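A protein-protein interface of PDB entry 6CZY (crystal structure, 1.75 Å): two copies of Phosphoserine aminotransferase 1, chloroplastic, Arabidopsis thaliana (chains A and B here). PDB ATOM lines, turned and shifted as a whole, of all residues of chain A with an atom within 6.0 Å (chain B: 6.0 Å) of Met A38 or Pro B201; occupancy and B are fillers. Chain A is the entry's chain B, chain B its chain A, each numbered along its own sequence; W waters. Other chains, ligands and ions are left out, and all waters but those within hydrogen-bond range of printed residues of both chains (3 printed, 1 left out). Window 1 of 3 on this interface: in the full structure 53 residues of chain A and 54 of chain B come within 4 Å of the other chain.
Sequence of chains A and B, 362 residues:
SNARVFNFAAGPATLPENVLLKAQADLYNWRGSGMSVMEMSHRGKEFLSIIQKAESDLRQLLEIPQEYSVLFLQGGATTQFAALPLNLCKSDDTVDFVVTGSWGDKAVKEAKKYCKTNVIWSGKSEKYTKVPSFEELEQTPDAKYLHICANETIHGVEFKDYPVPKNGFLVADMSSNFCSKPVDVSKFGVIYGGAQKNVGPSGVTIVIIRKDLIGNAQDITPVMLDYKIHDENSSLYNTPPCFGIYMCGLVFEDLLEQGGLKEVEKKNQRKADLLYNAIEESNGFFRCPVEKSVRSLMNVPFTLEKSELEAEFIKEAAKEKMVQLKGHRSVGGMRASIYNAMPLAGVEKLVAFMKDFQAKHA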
ATOM      1  N   LEU A  27      36.207 -26.762  17.944  1.00  0.00           N
ATOM      2  CA  LEU A  27      35.559 -26.117  19.095  1.00  0.00           C
ATOM      3  C   LEU A  27      36.466 -25.181  19.909  1.00  0.00           C
ATOM      4  O   LEU A  27      36.054 -24.076  20.317  1.00  0.00           O
ATOM      5  CB  LEU A  27      34.936 -27.165  20.026  1.00  0.00           C
ATOM      6  CG  LEU A  27      33.829 -26.615  20.929  1.00  0.00           C
ATOM      7  CD1 LEU A  27      32.555 -26.509  20.130  1.00  0.00           C
ATOM      8  CD2 LEU A  27      33.609 -27.446  22.172  1.00  0.00           C
ATOM      9  N   SER A  36      37.228 -20.041  20.030  1.00  0.00           N
ATOM     10  CA  SER A  36      36.062 -20.806  19.622  1.00  0.00           C
ATOM     11  C   SER A  36      35.089 -19.927  18.855  1.00  0.00           C
ATOM     12  O   SER A  36      35.038 -18.711  19.091  1.00  0.00           O
ATOM     13  CB  SER A  36      35.348 -21.362  20.849  1.00  0.00           C
ATOM     14  OG  SER A  36      34.216 -22.132  20.482  1.00  0.00           O
ATOM     15  N   VAL A  37      34.307 -20.536  17.956  1.00  0.00           N
ATOM     16  CA  VAL A  37      33.115 -19.846  17.447  1.00  0.00           C
ATOM     17  C   VAL A  37      32.263 -19.278  18.586  1.00  0.00           C
ATOM     18  O   VAL A  37      31.731 -18.174  18.467  1.00  0.00           O
ATOM     19  CB  VAL A  37      32.288 -20.766  16.561  1.00  0.00           C
ATOM     20  CG1 VAL A  37      30.938 -20.135  16.214  1.00  0.00           C
ATOM     21  CG2 VAL A  37      33.011 -21.047  15.279  1.00  0.00           C
ATOM     22  N   MET A  38      32.147 -20.005  19.708  1.00  0.00           N
ATOM     23  CA  MET A  38      31.365 -19.528  20.863  1.00  0.00           C
ATOM     24  C   MET A  38      31.864 -18.260  21.525  1.00  0.00           C
ATOM     25  O   MET A  38      31.131 -17.693  22.321  1.00  0.00           O
ATOM     26  CB  MET A  38      31.265 -20.610  21.938  1.00  0.00           C
ATOM     27  CG  MET A  38      30.281 -21.658  21.505  1.00  0.00           C
ATOM     28  SD  MET A  38      29.995 -22.917  22.788  1.00  0.00           S
ATOM     29  CE  MET A  38      31.340 -24.018  22.527  1.00  0.00           C
ATOM     30  N   GLU A  39      33.079 -17.810  21.158  1.00  0.00           N
ATOM     31  CA  GLU A  39      33.719 -16.638  21.753  1.00  0.00           C
ATOM     32  C   GLU A  39      33.941 -15.480  20.774  1.00  0.00           C
ATOM     33  O   GLU A  39      34.539 -14.474  21.162  1.00  0.00           O
ATOM     34  CB  GLU A  39      35.105 -17.066  22.301  1.00  0.00           C
ATOM     35  CG  GLU A  39      35.074 -18.197  23.356  1.00  0.00           C
ATOM     36  CD  GLU A  39      36.475 -18.685  23.646  1.00  0.00           C
ATOM     37  OE1 GLU A  39      37.080 -19.207  22.678  1.00  0.00           O
ATOM     38  OE2 GLU A  39      36.989 -18.523  24.780  1.00  0.00           O
ATOM     39  N   MET A  40      33.473 -15.638  19.516  1.00  0.00           N
ATOM     40  CA  MET A  40      33.742 -14.666  18.468  1.00  0.00           C
ATOM     41  C   MET A  40      32.777 -13.479  18.611  1.00  0.00           C
ATOM     42  O   MET A  40      31.592 -13.656  18.855  1.00  0.00           O
ATOM     43  CB  MET A  40      33.493 -15.254  17.086  1.00  0.00           C
ATOM     44  CG  MET A  40      34.524 -16.241  16.622  1.00  0.00           C
ATOM     45  SD  MET A  40      34.059 -17.003  15.061  1.00  0.00           S
ATOM     46  CE  MET A  40      35.496 -18.078  14.917  1.00  0.00           C
ATOM     47  N   CYS A 242      25.283 -17.355  17.455  1.00  0.00           N
ATOM     48  CA  CYS A 242      26.437 -17.566  16.564  1.00  0.00           C
ATOM     49  C   CYS A 242      26.804 -19.043  16.375  1.00  0.00           C
ATOM     50  O   CYS A 242      27.046 -19.468  15.241  1.00  0.00           O
ATOM     51  CB  CYS A 242      27.685 -16.806  17.048  1.00  0.00           C
ATOM     52  SG  CYS A 242      27.556 -14.971  17.106  1.00  0.00           S
ATOM     53  N   PHE A 243      26.934 -19.777  17.472  1.00  0.00           N
ATOM     54  CA  PHE A 243      27.322 -21.179  17.377  1.00  0.00           C
ATOM     55  C   PHE A 243      26.256 -21.994  16.637  1.00  0.00           C
ATOM     56  O   PHE A 243      26.560 -22.863  15.821  1.00  0.00           O
ATOM     57  CB  PHE A 243      27.563 -21.790  18.755  1.00  0.00           C
ATOM     58  CG  PHE A 243      28.225 -23.108  18.696  1.00  0.00           C
ATOM     59  CD1 PHE A 243      29.535 -23.198  18.291  1.00  0.00           C
ATOM     60  CD2 PHE A 243      27.527 -24.296  19.027  1.00  0.00           C
ATOM     61  CE1 PHE A 243      30.176 -24.443  18.203  1.00  0.00           C
ATOM     62  CE2 PHE A 243      28.169 -25.531  18.919  1.00  0.00           C
ATOM     63  CZ  PHE A 243      29.483 -25.603  18.528  1.00  0.00           C
ATOM     64  N   PRO B  12      29.653 -11.594  21.965  1.00  0.00           N
ATOM     65  CA  PRO B  12      30.141 -12.722  22.742  1.00  0.00           C
ATOM     66  C   PRO B  12      31.595 -12.509  23.161  1.00  0.00           C
ATOM     67  O   PRO B  12      32.262 -11.593  22.687  1.00  0.00           O
ATOM     68  CB  PRO B  12      29.988 -13.911  21.781  1.00  0.00           C
ATOM     69  CG  PRO B  12      28.877 -13.471  20.849  1.00  0.00           C
ATOM     70  CD  PRO B  12      29.210 -12.034  20.631  1.00  0.00           C
ATOM     71  N   ALA B  13      32.007 -13.307  24.115  1.00  0.00           N
ATOM     72  CA  ALA B  13      33.253 -13.074  24.865  1.00  0.00           C
ATOM     73  C   ALA B  13      34.034 -14.356  25.088  1.00  0.00           C
ATOM     74  O   ALA B  13      33.566 -15.485  24.853  1.00  0.00           O
ATOM     75  CB  ALA B  13      32.910 -12.465  26.200  1.00  0.00           C
ATOM     76  N   LEU B  15      35.640 -17.450  27.001  1.00  0.00           N
ATOM     77  CA  LEU B  15      35.072 -18.425  27.913  1.00  0.00           C
ATOM     78  C   LEU B  15      36.197 -19.271  28.558  1.00  0.00           C
ATOM     79  O   LEU B  15      37.313 -19.338  28.035  1.00  0.00           O
ATOM     80  CB  LEU B  15      34.150 -19.383  27.163  1.00  0.00           C
ATOM     81  CG  LEU B  15      32.859 -18.722  26.698  1.00  0.00           C
ATOM     82  CD1 LEU B  15      32.095 -19.518  25.621  1.00  0.00           C
ATOM     83  CD2 LEU B  15      31.978 -18.482  27.919  1.00  0.00           C
ATOM     84  N   LEU B  20      35.489 -25.121  27.691  1.00  0.00           N
ATOM     85  CA  LEU B  20      35.554 -25.464  26.250  1.00  0.00           C
ATOM     86  C   LEU B  20      36.071 -26.891  26.037  1.00  0.00           C
ATOM     87  O   LEU B  20      35.571 -27.637  25.217  1.00  0.00           O
ATOM     88  CB  LEU B  20      36.426 -24.473  25.449  1.00  0.00           C
ATOM     89  CG  LEU B  20      35.919 -23.033  25.489  1.00  0.00           C
ATOM     90  CD1 LEU B  20      36.979 -22.093  24.998  1.00  0.00           C
ATOM     91  CD2 LEU B  20      34.671 -22.881  24.661  1.00  0.00           C
ATOM     92  N   ALA B  23      33.407 -29.462  26.928  1.00  0.00           N
ATOM     93  CA  ALA B  23      32.451 -29.506  25.788  1.00  0.00           C
ATOM     94  C   ALA B  23      33.007 -30.256  24.591  1.00  0.00           C
ATOM     95  O   ALA B  23      32.303 -31.052  23.960  1.00  0.00           O
ATOM     96  CB  ALA B  23      32.017 -28.109  25.410  1.00  0.00           C
ATOM     97  N   ALA B 195      23.572 -14.334  28.157  1.00  0.00           N
ATOM     98  CA  ALA B 195      24.661 -15.151  28.722  1.00  0.00           C
ATOM     99  C   ALA B 195      26.021 -14.782  28.168  1.00  0.00           C
ATOM    100  O   ALA B 195      27.048 -14.999  28.838  1.00  0.00           O
ATOM    101  CB  ALA B 195      24.418 -16.613  28.432  1.00  0.00           C
ATOM    102  N   GLN B 196      26.028 -14.221  26.975  1.00  0.00           N
ATOM    103  CA  GLN B 196      27.210 -14.099  26.173  1.00  0.00           C
ATOM    104  C   GLN B 196      28.376 -13.205  26.668  1.00  0.00           C
ATOM    105  O   GLN B 196      29.298 -12.974  25.905  1.00  0.00           O
ATOM    106  CB  GLN B 196      26.821 -13.755  24.730  1.00  0.00           C
ATOM    107  CG  GLN B 196      26.260 -12.363  24.514  1.00  0.00           C
ATOM    108  CD  GLN B 196      24.749 -12.292  24.602  1.00  0.00           C
ATOM    109  OE1 GLN B 196      24.091 -13.160  25.211  1.00  0.00           O
ATOM    110  NE2 GLN B 196      24.189 -11.250  24.002  1.00  0.00           N
ATOM    111  N   VAL B 199      28.634 -15.816  31.206  1.00  0.00           N
ATOM    112  CA  VAL B 199      28.216 -17.147  31.613  1.00  0.00           C
ATOM    113  C   VAL B 199      27.977 -18.194  30.527  1.00  0.00           C
ATOM    114  O   VAL B 199      27.633 -19.334  30.863  1.00  0.00           O
ATOM    115  CB  VAL B 199      27.056 -17.103  32.586  1.00  0.00           C
ATOM    116  CG1 VAL B 199      27.450 -16.287  33.807  1.00  0.00           C
ATOM    117  CG2 VAL B 199      25.830 -16.468  31.945  1.00  0.00           C
ATOM    118  N   GLY B 200      28.237 -17.858  29.259  1.00  0.00           N
ATOM    119  CA  GLY B 200      27.979 -18.768  28.161  1.00  0.00           C
ATOM    120  C   GLY B 200      28.072 -18.149  26.800  1.00  0.00           C
ATOM    121  O   GLY B 200      28.567 -17.002  26.640  1.00  0.00           O
ATOM    122  N   PRO B 201      27.607 -18.899  25.788  1.00  0.00           N
ATOM    123  CA  PRO B 201      27.573 -18.383  24.431  1.00  0.00           C
ATOM    124  C   PRO B 201      26.296 -17.628  24.160  1.00  0.00           C
ATOM    125  O   PRO B 201      25.402 -17.612  24.983  1.00  0.00           O
ATOM    126  CB  PRO B 201      27.610 -19.648  23.576  1.00  0.00           C
ATOM    127  CG  PRO B 201      26.842 -20.652  24.379  1.00  0.00           C
ATOM    128  CD  PRO B 201      27.172 -20.311  25.839  1.00  0.00           C
ATOM    129  N   SER B 202      26.249 -16.938  23.043  1.00  0.00           N
ATOM    130  CA  SER B 202      25.046 -16.209  22.672  1.00  0.00           C
ATOM    131  C   SER B 202      23.958 -17.189  22.334  1.00  0.00           C
ATOM    132  O   SER B 202      24.234 -18.266  21.853  1.00  0.00           O
ATOM    133  CB  SER B 202      25.309 -15.235  21.528  1.00  0.00           C
ATOM    134  OG  SER B 202      25.845 -15.893  20.395  1.00  0.00           O
ATOM    135  N   GLY B 203      22.714 -16.803  22.600  1.00  0.00           N
ATOM    136  CA  GLY B 203      21.580 -17.676  22.329  1.00  0.00           C
ATOM    137  C   GLY B 203      20.734 -17.989  23.540  1.00  0.00           C
ATOM    138  O   GLY B 203      19.616 -18.513  23.383  1.00  0.00           O
ATOM    139  N   VAL B 204      21.251 -17.683  24.728  1.00  0.00           N
ATOM    140  CA  VAL B 204      20.552 -17.891  25.961  1.00  0.00           C
ATOM    141  C   VAL B 204      20.495 -16.543  26.709  1.00  0.00           C
ATOM    142  O   VAL B 204      21.504 -15.794  26.755  1.00  0.00           O
ATOM    143  CB  VAL B 204      21.297 -18.899  26.873  1.00  0.00           C
ATOM    144  CG1 VAL B 204      20.561 -19.063  28.202  1.00  0.00           C
ATOM    145  CG2 VAL B 204      21.458 -20.213  26.183  1.00  0.00           C
ATOM    146  N   PHE B 243      21.809 -26.625  23.796  1.00  0.00           N
ATOM    147  CA  PHE B 243      23.261 -26.573  23.890  1.00  0.00           C
ATOM    148  C   PHE B 243      23.775 -25.341  24.641  1.00  0.00           C
ATOM    149  O   PHE B 243      24.710 -25.447  25.460  1.00  0.00           O
ATOM    150  CB  PHE B 243      23.902 -26.700  22.526  1.00  0.00           C
ATOM    151  CG  PHE B 243      25.372 -26.900  22.589  1.00  0.00           C
ATOM    152  CD1 PHE B 243      25.902 -28.152  22.954  1.00  0.00           C
ATOM    153  CD2 PHE B 243      26.239 -25.866  22.293  1.00  0.00           C
ATOM    154  CE1 PHE B 243      27.271 -28.334  23.062  1.00  0.00           C
ATOM    155  CE2 PHE B 243      27.613 -26.067  22.354  1.00  0.00           C
ATOM    156  CZ  PHE B 243      28.119 -27.270  22.757  1.00  0.00           C
ATOM    157  N   GLY B 244      23.176 -24.169  24.377  1.00  0.00           N
ATOM    158  CA  GLY B 244      23.543 -22.977  25.120  1.00  0.00           C
ATOM    159  C   GLY B 244      23.324 -23.151  26.618  1.00  0.00           C
ATOM    160  O   GLY B 244      24.136 -22.683  27.432  1.00  0.00           O
ATOM    161  N   MET B 247      26.030 -25.274  27.997  1.00  0.00           N
ATOM    162  CA  MET B 247      27.241 -24.503  28.166  1.00  0.00           C
ATOM    163  C   MET B 247      27.191 -23.589  29.397  1.00  0.00           C
ATOM    164  O   MET B 247      28.182 -23.546  30.175  1.00  0.00           O
ATOM    165  CB  MET B 247      27.564 -23.702  26.896  1.00  0.00           C
ATOM    166  CG  MET B 247      27.907 -24.582  25.722  1.00  0.00           C
ATOM    167  SD  MET B 247      29.430 -25.523  25.902  1.00  0.00           S
ATOM    168  CE  MET B 247      30.566 -24.245  26.363  1.00  0.00           C
ATOM    169  N   CYS B 248      26.063 -22.881  29.600  1.00  0.00           N
ATOM    170  CA  CYS B 248      25.907 -22.057  30.787  1.00  0.00           C
ATOM    171  C   CYS B 248      26.079 -22.924  32.072  1.00  0.00           C
ATOM    172  O   CYS B 248      26.758 -22.535  33.062  1.00  0.00           O
ATOM    173  CB  CYS B 248      24.531 -21.390  30.834  1.00  0.00           C
ATOM    174  SG  CYS B 248      24.314 -20.115  29.581  1.00  0.00           S
HETATM  175  O   HOH W   1      24.056 -20.284  19.390  1.00  0.00           O
HETATM  176  O   HOH W   2      26.729 -18.789  20.228  1.00  0.00           O
HETATM  177  O   HOH W   3      28.744 -17.119  21.301  1.00  0.00           O
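Among the printed residues, pairs that only touch across the chains: Leu A27 with Leu B20 (3.6 Å), Leu A27 with Ala B23 (3.7 Å), Met A38 with Pro B12 (3.99 Å), Met A38 with Leu B15 (3.9 Å), Met A38 with Pro B201 (3.9 Å), Met A38 with Phe B243 (3.97 Å), Met A38 with Met B247 (3.9 Å), Glu A39 with Pro B12 (3.98 Å), Glu A39 with Ala B13 (3.3 Å), Glu A39 with Leu B20 (3.6 Å), Met A40 with Pro B12 (3.3 Å) and Phe A243 with Phe B243 (3.5 Å).
Printed residues of chain B that touch a printed residue of chain A: Pro B12, Ala B13, Leu B15, Leu B20, Ala B23, Pro B201, Ser B202, Phe B243 and Met B247.
Hydrophobic or aromatic side chains of chain B within 4 Å of the printed part of chain A: Pro B12, Leu B15, Leu B20, Ala B23, Pro B201, Phe B243 and Met B247.
Along chain B the printed residues that touch a printed residue of chain A span positions 12 to 247.
Of the 8 printed residues of chain A, 6 touch a printed residue of chain B.
Among the printed residues, 14 pairs touch across the chains.
Among the printed residues, no Asp or Glu carboxylate lies within 4 Å of a Lys or Arg side-chain nitrogen of the other chain.
Phe A243 touches its own counterpart, Phe B243.
1 position is printed for both chains.
Printed residues of chain B within 4 Å of Met A38: Pro B12 (3.99 Å), Leu B15 (3.9 Å), Pro B201 (3.9 Å), Phe B243 (3.97 Å) and Met B247 (3.9 Å).
Pro B201 touches just one residue of chain A: Met A38 (3.9 Å).
Of the printed residues of chain A, Met B247 touches Met A38.
Printed residues of chain A within 4 Å of Leu B15: Met A38 (3.9 Å) and Glu A39 (2.8 Å).
Printed residues of chain B within 4 Å of Leu A27: Leu B20 (3.6 Å) and Ala B23 (3.7 Å).
Of the printed residues of chain A, Ala B13 touches Glu A39 (3.3 Å).
The nearest residue of chain A that does not touch Pro B201 is Phe A243 (5.3 Å).
The backbone carbonyl oxygen (O) of Leu A27 lies within hydrogen-bond range of the side-chain hydroxyl (OG) of Ser A36.
The backbone carbonyl oxygen (O) of Gln B196 is in hydrogen-bond range of the backbone NH (N) of Ala B13 (3.3 Å).
The side-chain hydroxyl (OG) of Ser A36 sits close to the backbone NH (N) of Met A38 (3.1 Å).
The side-chain carboxylate (OE1) of Glu A39 sits at hydrogen-bond distance from the backbone NH (N) of Ser A36 (2.8 Å).
Water W3 lies within hydrogen-bond range of O of Met A38 (2.7 Å) and N of Ser B202 (3.0 Å).
Water W2 lies within hydrogen-bond range of N of Phe A243 (2.9 Å), O of Ser B202 (3.0 Å) and N of Cys A242 (3.4 Å).
Water W1 lies within hydrogen-bond range of the backbone carbonyl oxygen of Ser B202 (3.2 Å) and the backbone NH of Phe A243 (3.5 Å).
The backbone NH of Leu B15 lies within hydrogen-bond range of the side-chain carboxylate of Glu A39, 2.8 Å away.
The backbone NH (N) of Cys A242 lies within hydrogen-bond range of the side-chain hydroxyl (OG) of Ser B202, at 3.3 Å.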
